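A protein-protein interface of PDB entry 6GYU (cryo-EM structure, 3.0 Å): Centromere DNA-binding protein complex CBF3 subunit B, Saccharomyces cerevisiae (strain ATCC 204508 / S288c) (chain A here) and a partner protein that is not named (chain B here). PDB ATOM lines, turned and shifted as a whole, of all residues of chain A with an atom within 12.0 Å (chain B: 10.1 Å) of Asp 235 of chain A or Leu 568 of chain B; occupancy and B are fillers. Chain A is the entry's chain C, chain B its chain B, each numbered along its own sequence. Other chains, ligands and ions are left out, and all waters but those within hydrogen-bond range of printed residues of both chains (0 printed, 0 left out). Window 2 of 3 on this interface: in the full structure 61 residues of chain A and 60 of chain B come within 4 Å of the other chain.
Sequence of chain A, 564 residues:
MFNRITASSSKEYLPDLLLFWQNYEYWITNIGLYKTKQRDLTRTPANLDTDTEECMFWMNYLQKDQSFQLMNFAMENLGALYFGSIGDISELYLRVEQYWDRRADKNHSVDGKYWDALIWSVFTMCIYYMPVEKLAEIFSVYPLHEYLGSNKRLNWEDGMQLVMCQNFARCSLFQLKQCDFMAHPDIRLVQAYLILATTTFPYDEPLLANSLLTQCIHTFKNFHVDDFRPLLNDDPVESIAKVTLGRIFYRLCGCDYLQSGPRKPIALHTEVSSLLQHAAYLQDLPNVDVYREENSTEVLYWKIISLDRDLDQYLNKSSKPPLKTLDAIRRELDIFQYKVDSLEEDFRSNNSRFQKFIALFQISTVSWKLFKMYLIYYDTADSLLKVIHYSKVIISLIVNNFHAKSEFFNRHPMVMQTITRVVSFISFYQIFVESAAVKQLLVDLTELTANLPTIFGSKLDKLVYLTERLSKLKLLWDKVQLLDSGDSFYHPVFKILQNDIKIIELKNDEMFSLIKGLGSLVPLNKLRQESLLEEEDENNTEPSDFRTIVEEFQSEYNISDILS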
ATOM      1  N   VAL A 225      -0.778  -2.222  27.769  1.00  0.00           N
ATOM      2  CA  VAL A 225      -1.793  -2.706  28.698  1.00  0.00           C
ATOM      3  C   VAL A 225      -1.521  -4.185  28.955  1.00  0.00           C
ATOM      4  O   VAL A 225      -1.711  -5.023  28.070  1.00  0.00           O
ATOM      5  CB  VAL A 225      -3.207  -2.483  28.150  1.00  0.00           C
ATOM      6  CG1 VAL A 225      -4.237  -3.099  29.076  1.00  0.00           C
ATOM      7  CG2 VAL A 225      -3.472  -1.001  27.969  1.00  0.00           C
ATOM      8  N   ASP A 227      -2.502  -6.103  32.213  1.00  0.00           N
ATOM      9  CA  ASP A 227      -3.654  -6.704  32.866  1.00  0.00           C
ATOM     10  C   ASP A 227      -4.925  -6.092  32.294  1.00  0.00           C
ATOM     11  O   ASP A 227      -4.990  -4.884  32.051  1.00  0.00           O
ATOM     12  CB  ASP A 227      -3.593  -6.492  34.382  1.00  0.00           C
ATOM     13  CG  ASP A 227      -4.555  -7.390  35.145  1.00  0.00           C
ATOM     14  OD1 ASP A 227      -5.272  -8.196  34.514  1.00  0.00           O
ATOM     15  OD2 ASP A 227      -4.593  -7.291  36.390  1.00  0.00           O
ATOM     16  N   PHE A 228      -5.935  -6.933  32.082  1.00  0.00           N
ATOM     17  CA  PHE A 228      -7.177  -6.508  31.453  1.00  0.00           C
ATOM     18  C   PHE A 228      -8.350  -6.521  32.425  1.00  0.00           C
ATOM     19  O   PHE A 228      -9.497  -6.330  32.012  1.00  0.00           O
ATOM     20  CB  PHE A 228      -7.478  -7.394  30.246  1.00  0.00           C
ATOM     21  CG  PHE A 228      -6.390  -7.394  29.220  1.00  0.00           C
ATOM     22  CD1 PHE A 228      -6.238  -6.327  28.351  1.00  0.00           C
ATOM     23  CD2 PHE A 228      -5.516  -8.462  29.125  1.00  0.00           C
ATOM     24  CE1 PHE A 228      -5.233  -6.328  27.409  1.00  0.00           C
ATOM     25  CE2 PHE A 228      -4.512  -8.468  28.187  1.00  0.00           C
ATOM     26  CZ  PHE A 228      -4.369  -7.401  27.329  1.00  0.00           C
ATOM     27  N   ARG A 229      -8.086  -6.742  33.704  1.00  0.00           N
ATOM     28  CA  ARG A 229      -9.143  -6.725  34.706  1.00  0.00           C
ATOM     29  C   ARG A 229      -9.501  -5.288  35.058  1.00  0.00           C
ATOM     30  O   ARG A 229      -8.602  -4.445  35.166  1.00  0.00           O
ATOM     31  CB  ARG A 229      -8.711  -7.472  35.957  1.00  0.00           C
ATOM     32  CG  ARG A 229      -8.542  -8.966  35.752  1.00  0.00           C
ATOM     33  CD  ARG A 229      -8.054  -9.638  37.018  1.00  0.00           C
ATOM     34  NE  ARG A 229      -6.691  -9.237  37.348  1.00  0.00           N
ATOM     35  CZ  ARG A 229      -6.074  -9.551  38.483  1.00  0.00           C
ATOM     36  NH1 ARG A 229      -6.702 -10.268  39.403  1.00  0.00           N
ATOM     37  NH2 ARG A 229      -4.832  -9.144  38.698  1.00  0.00           N
ATOM     38  N   PRO A 230     -10.786  -4.971  35.221  1.00  0.00           N
ATOM     39  CA  PRO A 230     -11.172  -3.586  35.514  1.00  0.00           C
ATOM     40  C   PRO A 230     -10.791  -3.176  36.928  1.00  0.00           C
ATOM     41  O   PRO A 230     -11.106  -3.863  37.903  1.00  0.00           O
ATOM     42  CB  PRO A 230     -12.696  -3.599  35.338  1.00  0.00           C
ATOM     43  CG  PRO A 230     -12.975  -4.795  34.488  1.00  0.00           C
ATOM     44  CD  PRO A 230     -11.953  -5.807  34.897  1.00  0.00           C
ATOM     45  N   LEU A 231     -10.102  -2.045  37.031  1.00  0.00           N
ATOM     46  CA  LEU A 231      -9.758  -1.471  38.320  1.00  0.00           C
ATOM     47  C   LEU A 231     -10.881  -0.558  38.806  1.00  0.00           C
ATOM     48  O   LEU A 231     -11.640   0.014  38.021  1.00  0.00           O
ATOM     49  CB  LEU A 231      -8.438  -0.704  38.231  1.00  0.00           C
ATOM     50  CG  LEU A 231      -7.186  -1.533  37.938  1.00  0.00           C
ATOM     51  CD1 LEU A 231      -5.978  -0.630  37.760  1.00  0.00           C
ATOM     52  CD2 LEU A 231      -6.940  -2.549  39.041  1.00  0.00           C
ATOM     53  N   LEU A 232     -10.978  -0.424  40.130  1.00  0.00           N
ATOM     54  CA  LEU A 232     -12.063   0.341  40.735  1.00  0.00           C
ATOM     55  C   LEU A 232     -11.886   1.847  40.583  1.00  0.00           C
ATOM     56  O   LEU A 232     -12.877   2.581  40.647  1.00  0.00           O
ATOM     57  CB  LEU A 232     -12.203  -0.005  42.224  1.00  0.00           C
ATOM     58  N   ASN A 233     -10.659   2.322  40.379  1.00  0.00           N
ATOM     59  CA  ASN A 233     -10.380   3.747  40.287  1.00  0.00           C
ATOM     60  C   ASN A 233     -10.471   4.299  38.870  1.00  0.00           C
ATOM     61  O   ASN A 233     -10.404   5.520  38.691  1.00  0.00           O
ATOM     62  CB  ASN A 233      -8.996   4.050  40.883  1.00  0.00           C
ATOM     63  N   ASP A 234     -10.621   3.441  37.867  1.00  0.00           N
ATOM     64  CA  ASP A 234     -10.580   3.892  36.487  1.00  0.00           C
ATOM     65  C   ASP A 234     -11.910   4.503  36.062  1.00  0.00           C
ATOM     66  O   ASP A 234     -12.954   4.298  36.687  1.00  0.00           O
ATOM     67  CB  ASP A 234     -10.222   2.736  35.550  1.00  0.00           C
ATOM     68  CG  ASP A 234      -8.780   2.293  35.692  1.00  0.00           C
ATOM     69  OD1 ASP A 234      -7.932   3.132  36.063  1.00  0.00           O
ATOM     70  OD2 ASP A 234      -8.491   1.109  35.423  1.00  0.00           O
ATOM     71  N   ASP A 235     -11.841   5.290  34.994  1.00  0.00           N
ATOM     72  CA  ASP A 235     -13.029   5.742  34.286  1.00  0.00           C
ATOM     73  C   ASP A 235     -13.760   4.519  33.733  1.00  0.00           C
ATOM     74  O   ASP A 235     -13.119   3.650  33.129  1.00  0.00           O
ATOM     75  CB  ASP A 235     -12.602   6.681  33.152  1.00  0.00           C
ATOM     76  CG  ASP A 235     -13.749   7.493  32.561  1.00  0.00           C
ATOM     77  OD1 ASP A 235     -14.902   7.376  33.012  1.00  0.00           O
ATOM     78  OD2 ASP A 235     -13.483   8.269  31.618  1.00  0.00           O
ATOM     79  N   PRO A 236     -15.078   4.393  33.941  1.00  0.00           N
ATOM     80  CA  PRO A 236     -15.812   3.237  33.393  1.00  0.00           C
ATOM     81  C   PRO A 236     -15.865   3.149  31.870  1.00  0.00           C
ATOM     82  O   PRO A 236     -16.382   2.154  31.353  1.00  0.00           O
ATOM     83  CB  PRO A 236     -17.218   3.415  33.980  1.00  0.00           C
ATOM     84  CG  PRO A 236     -16.987   4.119  35.256  1.00  0.00           C
ATOM     85  CD  PRO A 236     -15.846   5.062  35.006  1.00  0.00           C
ATOM     86  N   VAL A 237     -15.365   4.138  31.128  1.00  0.00           N
ATOM     87  CA  VAL A 237     -15.091   3.931  29.711  1.00  0.00           C
ATOM     88  C   VAL A 237     -13.786   3.161  29.538  1.00  0.00           C
ATOM     89  O   VAL A 237     -13.695   2.240  28.716  1.00  0.00           O
ATOM     90  CB  VAL A 237     -15.061   5.287  28.981  1.00  0.00           C
ATOM     91  CG1 VAL A 237     -14.746   5.106  27.505  1.00  0.00           C
ATOM     92  CG2 VAL A 237     -16.379   6.017  29.166  1.00  0.00           C
ATOM     93  N   GLU A 238     -12.775   3.503  30.345  1.00  0.00           N
ATOM     94  CA  GLU A 238     -11.462   2.870  30.258  1.00  0.00           C
ATOM     95  C   GLU A 238     -11.499   1.403  30.677  1.00  0.00           C
ATOM     96  O   GLU A 238     -10.760   0.585  30.117  1.00  0.00           O
ATOM     97  CB  GLU A 238     -10.465   3.652  31.117  1.00  0.00           C
ATOM     98  CG  GLU A 238      -9.030   3.159  31.066  1.00  0.00           C
ATOM     99  CD  GLU A 238      -8.093   4.006  31.906  1.00  0.00           C
ATOM    100  OE1 GLU A 238      -8.567   4.979  32.528  1.00  0.00           O
ATOM    101  OE2 GLU A 238      -6.883   3.695  31.947  1.00  0.00           O
ATOM    102  N   SER A 239     -12.366   1.043  31.627  1.00  0.00           N
ATOM    103  CA  SER A 239     -12.459  -0.353  32.046  1.00  0.00           C
ATOM    104  C   SER A 239     -13.085  -1.220  30.959  1.00  0.00           C
ATOM    105  O   SER A 239     -12.613  -2.334  30.695  1.00  0.00           O
ATOM    106  CB  SER A 239     -13.259  -0.461  33.342  1.00  0.00           C
ATOM    107  OG  SER A 239     -14.612  -0.099  33.132  1.00  0.00           O
ATOM    108  N   ILE A 240     -14.134  -0.713  30.303  1.00  0.00           N
ATOM    109  CA  ILE A 240     -14.736  -1.417  29.173  1.00  0.00           C
ATOM    110  C   ILE A 240     -13.749  -1.487  28.012  1.00  0.00           C
ATOM    111  O   ILE A 240     -13.684  -2.491  27.289  1.00  0.00           O
ATOM    112  CB  ILE A 240     -16.062  -0.736  28.778  1.00  0.00           C
ATOM    113  CG1 ILE A 240     -17.055  -0.818  29.938  1.00  0.00           C
ATOM    114  CG2 ILE A 240     -16.688  -1.373  27.547  1.00  0.00           C
ATOM    115  CD1 ILE A 240     -18.316  -0.012  29.725  1.00  0.00           C
ATOM    116  N   ALA A 241     -12.916  -0.454  27.866  1.00  0.00           N
ATOM    117  CA  ALA A 241     -11.876  -0.461  26.843  1.00  0.00           C
ATOM    118  C   ALA A 241     -10.806  -1.516  27.122  1.00  0.00           C
ATOM    119  O   ALA A 241     -10.319  -2.176  26.197  1.00  0.00           O
ATOM    120  CB  ALA A 241     -11.255   0.927  26.748  1.00  0.00           C
ATOM    121  N   LYS A 242     -10.441  -1.706  28.392  1.00  0.00           N
ATOM    122  CA  LYS A 242      -9.462  -2.737  28.723  1.00  0.00           C
ATOM    123  C   LYS A 242     -10.049  -4.140  28.608  1.00  0.00           C
ATOM    124  O   LYS A 242      -9.330  -5.079  28.252  1.00  0.00           O
ATOM    125  CB  LYS A 242      -8.897  -2.510  30.123  1.00  0.00           C
ATOM    126  CG  LYS A 242      -8.005  -1.289  30.226  1.00  0.00           C
ATOM    127  CD  LYS A 242      -7.287  -1.234  31.560  1.00  0.00           C
ATOM    128  CE  LYS A 242      -8.228  -0.840  32.681  1.00  0.00           C
ATOM    129  NZ  LYS A 242      -7.500  -0.661  33.966  1.00  0.00           N
ATOM    130  N   VAL A 243     -11.347  -4.301  28.878  1.00  0.00           N
ATOM    131  CA  VAL A 243     -12.005  -5.584  28.621  1.00  0.00           C
ATOM    132  C   VAL A 243     -12.053  -5.869  27.119  1.00  0.00           C
ATOM    133  O   VAL A 243     -11.874  -7.018  26.675  1.00  0.00           O
ATOM    134  CB  VAL A 243     -13.405  -5.588  29.268  1.00  0.00           C
ATOM    135  CG1 VAL A 243     -14.213  -6.812  28.869  1.00  0.00           C
ATOM    136  CG2 VAL A 243     -13.274  -5.546  30.776  1.00  0.00           C
ATOM    137  N   THR A 244     -12.245  -4.819  26.313  1.00  0.00           N
ATOM    138  CA  THR A 244     -12.204  -4.955  24.861  1.00  0.00           C
ATOM    139  C   THR A 244     -10.817  -5.367  24.382  1.00  0.00           C
ATOM    140  O   THR A 244     -10.692  -6.256  23.534  1.00  0.00           O
ATOM    141  CB  THR A 244     -12.634  -3.644  24.205  1.00  0.00           C
ATOM    142  OG1 THR A 244     -13.941  -3.290  24.670  1.00  0.00           O
ATOM    143  CG2 THR A 244     -12.684  -3.788  22.698  1.00  0.00           C
ATOM    144  N   MET B 555      -3.937   5.384  25.704  1.00  0.00           N
ATOM    145  CA  MET B 555      -5.284   5.001  26.109  1.00  0.00           C
ATOM    146  C   MET B 555      -6.335   5.909  25.481  1.00  0.00           C
ATOM    147  O   MET B 555      -7.439   5.454  25.170  1.00  0.00           O
ATOM    148  CB  MET B 555      -5.391   5.018  27.635  1.00  0.00           C
ATOM    149  CG  MET B 555      -6.708   4.501  28.194  1.00  0.00           C
ATOM    150  SD  MET B 555      -7.015   2.772  27.787  1.00  0.00           S
ATOM    151  CE  MET B 555      -5.832   1.960  28.853  1.00  0.00           C
ATOM    152  N   PHE B 556      -6.005   7.183  25.260  1.00  0.00           N
ATOM    153  CA  PHE B 556      -6.971   8.095  24.657  1.00  0.00           C
ATOM    154  C   PHE B 556      -7.182   7.797  23.180  1.00  0.00           C
ATOM    155  O   PHE B 556      -8.322   7.820  22.703  1.00  0.00           O
ATOM    156  CB  PHE B 556      -6.519   9.538  24.859  1.00  0.00           C
ATOM    157  CG  PHE B 556      -6.524   9.971  26.295  1.00  0.00           C
ATOM    158  CD1 PHE B 556      -7.702  10.368  26.909  1.00  0.00           C
ATOM    159  CD2 PHE B 556      -5.351   9.968  27.035  1.00  0.00           C
ATOM    160  CE1 PHE B 556      -7.710  10.762  28.234  1.00  0.00           C
ATOM    161  CE2 PHE B 556      -5.351  10.361  28.360  1.00  0.00           C
ATOM    162  CZ  PHE B 556      -6.531  10.759  28.961  1.00  0.00           C
ATOM    163  N   ILE B 559      -9.385   4.724  23.137  1.00  0.00           N
ATOM    164  CA  ILE B 559     -10.799   5.037  23.350  1.00  0.00           C
ATOM    165  C   ILE B 559     -11.397   5.681  22.104  1.00  0.00           C
ATOM    166  O   ILE B 559     -12.536   5.385  21.717  1.00  0.00           O
ATOM    167  CB  ILE B 559     -10.951   5.924  24.603  1.00  0.00           C
ATOM    168  CG1 ILE B 559     -10.595   5.131  25.859  1.00  0.00           C
ATOM    169  CG2 ILE B 559     -12.349   6.484  24.745  1.00  0.00           C
ATOM    170  CD1 ILE B 559     -10.454   5.985  27.095  1.00  0.00           C
ATOM    171  N   LYS B 560     -10.621   6.530  21.425  1.00  0.00           N
ATOM    172  CA  LYS B 560     -11.084   7.106  20.166  1.00  0.00           C
ATOM    173  C   LYS B 560     -11.145   6.067  19.053  1.00  0.00           C
ATOM    174  O   LYS B 560     -11.901   6.236  18.091  1.00  0.00           O
ATOM    175  CB  LYS B 560     -10.179   8.266  19.756  1.00  0.00           C
ATOM    176  CG  LYS B 560     -10.285   9.485  20.656  1.00  0.00           C
ATOM    177  CD  LYS B 560      -9.347  10.587  20.198  1.00  0.00           C
ATOM    178  CE  LYS B 560      -9.417  11.793  21.122  1.00  0.00           C
ATOM    179  NZ  LYS B 560      -8.492  12.876  20.689  1.00  0.00           N
ATOM    180  N   SER B 564     -17.413   5.335  19.188  1.00  0.00           N
ATOM    181  CA  SER B 564     -17.835   6.703  19.464  1.00  0.00           C
ATOM    182  C   SER B 564     -17.637   7.028  20.938  1.00  0.00           C
ATOM    183  O   SER B 564     -18.315   7.903  21.488  1.00  0.00           O
ATOM    184  CB  SER B 564     -19.298   6.907  19.065  1.00  0.00           C
ATOM    185  OG  SER B 564     -19.471   6.761  17.667  1.00  0.00           O
ATOM    186  N   LEU B 565     -16.714   6.322  21.584  1.00  0.00           N
ATOM    187  CA  LEU B 565     -16.438   6.544  22.994  1.00  0.00           C
ATOM    188  C   LEU B 565     -15.641   7.828  23.175  1.00  0.00           C
ATOM    189  O   LEU B 565     -14.658   8.073  22.471  1.00  0.00           O
ATOM    190  CB  LEU B 565     -15.672   5.354  23.569  1.00  0.00           C
ATOM    191  CG  LEU B 565     -16.377   3.998  23.535  1.00  0.00           C
ATOM    192  CD1 LEU B 565     -15.443   2.902  24.025  1.00  0.00           C
ATOM    193  CD2 LEU B 565     -17.659   4.029  24.351  1.00  0.00           C
ATOM    194  N   VAL B 566     -16.072   8.651  24.124  1.00  0.00           N
ATOM    195  CA  VAL B 566     -15.478   9.957  24.381  1.00  0.00           C
ATOM    196  C   VAL B 566     -14.864   9.923  25.773  1.00  0.00           C
ATOM    197  O   VAL B 566     -15.568   9.627  26.740  1.00  0.00           O
ATOM    198  CB  VAL B 566     -16.504  11.100  24.278  1.00  0.00           C
ATOM    199  CG1 VAL B 566     -15.862  12.426  24.648  1.00  0.00           C
ATOM    200  CG2 VAL B 566     -17.093  11.156  22.877  1.00  0.00           C
ATOM    201  N   PRO B 567     -13.568  10.200  25.923  1.00  0.00           N
ATOM    202  CA  PRO B 567     -12.968  10.221  27.264  1.00  0.00           C
ATOM    203  C   PRO B 567     -13.406  11.453  28.045  1.00  0.00           C
ATOM    204  O   PRO B 567     -13.257  12.588  27.586  1.00  0.00           O
ATOM    205  CB  PRO B 567     -11.461  10.228  26.979  1.00  0.00           C
ATOM    206  CG  PRO B 567     -11.338  10.819  25.613  1.00  0.00           C
ATOM    207  CD  PRO B 567     -12.565  10.390  24.859  1.00  0.00           C
ATOM    208  N   LEU B 568     -13.963  11.217  29.234  1.00  0.00           N
ATOM    209  CA  LEU B 568     -14.463  12.284  30.092  1.00  0.00           C
ATOM    210  C   LEU B 568     -13.351  13.000  30.848  1.00  0.00           C
ATOM    211  O   LEU B 568     -13.562  14.115  31.342  1.00  0.00           O
ATOM    212  CB  LEU B 568     -15.498  11.726  31.070  1.00  0.00           C
ATOM    213  N   ASN B 569     -12.174  12.394  30.948  1.00  0.00           N
ATOM    214  CA  ASN B 569     -11.054  13.005  31.655  1.00  0.00           C
ATOM    215  C   ASN B 569      -9.768  12.894  30.843  1.00  0.00           C
ATOM    216  O   ASN B 569      -9.366  13.839  30.166  1.00  0.00           O
ATOM    217  CB  ASN B 569     -10.869  12.356  33.029  1.00  0.00           C
ATOM    218  CG  ASN B 569     -11.987  12.703  33.993  1.00  0.00           C
ATOM    219  OD1 ASN B 569     -12.429  13.850  34.062  1.00  0.00           O
ATOM    220  ND2 ASN B 569     -12.451  11.709  34.743  1.00  0.00           N
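Val 225 of chain A touches Met 555 of chain B (CG2 to CE, 3.9 Å). Asp 235 of chain A touches Leu 568 of chain B (OD2 to N, 3.8 Å). CG1 of Val 237 of chain A touches CG2 of Ile 559 of chain B (3.9 Å). OE2 of Glu 238 of chain A touches CE of Met 555 of chain B (3.7 Å).
Asp 235 of chain A touches just one residue of chain B: Leu 568. Of chain A, only Asp 235 comes within 4 Å of Leu 568 of chain B. Val 237 of chain A touches one residue of chain B. Glu 238 of chain A touches just one residue of chain B: Met 555 (3.7 Å). No residue of chain A comes within 4 Å of Pro 567 of chain B. Of the printed residues of chain A, Met 555 of chain B touches Val 225 (3.9 Å) and Glu 238 (3.7 Å). Of the printed residues of chain A, Ile 559 of chain B touches Val 237 (3.9 Å). Printed residues of chain B within 4 Å of Val 225 of chain A: Met 555 (3.9 Å). Phe 556 of chain B touches none of the printed residues of chain A. The nearest residue of chain B that does not touch Asp 235 of chain A is Asn 569 of chain B (4.4 Å). The nearest printed residue of chain B that does not touch Val 225 of chain A is Phe 556 of chain B (9.0 Å).
Of the 19 printed residues of chain A, 4 touch a printed residue of chain B. Printed residues of chain A that touch a printed residue of chain B: Val 225, Asp 235, Val 237 and Glu 238. Hydrophobic or aromatic side chains of chain A within 4 Å of the printed part of chain B: Val 225 and Val 237. Hydrophobic or aromatic side chains of chain B within 4 Å of the printed part of chain A: Met 555 and Ile 559. Along chain B the printed residues that touch a printed residue of chain A span positions 555 to 568. Among the printed residues, 4 pairs touch across the chains. Among the printed residues, no Asp or Glu carboxylate lies within 4 Å of a Lys or Arg side-chain nitrogen of the other chain.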
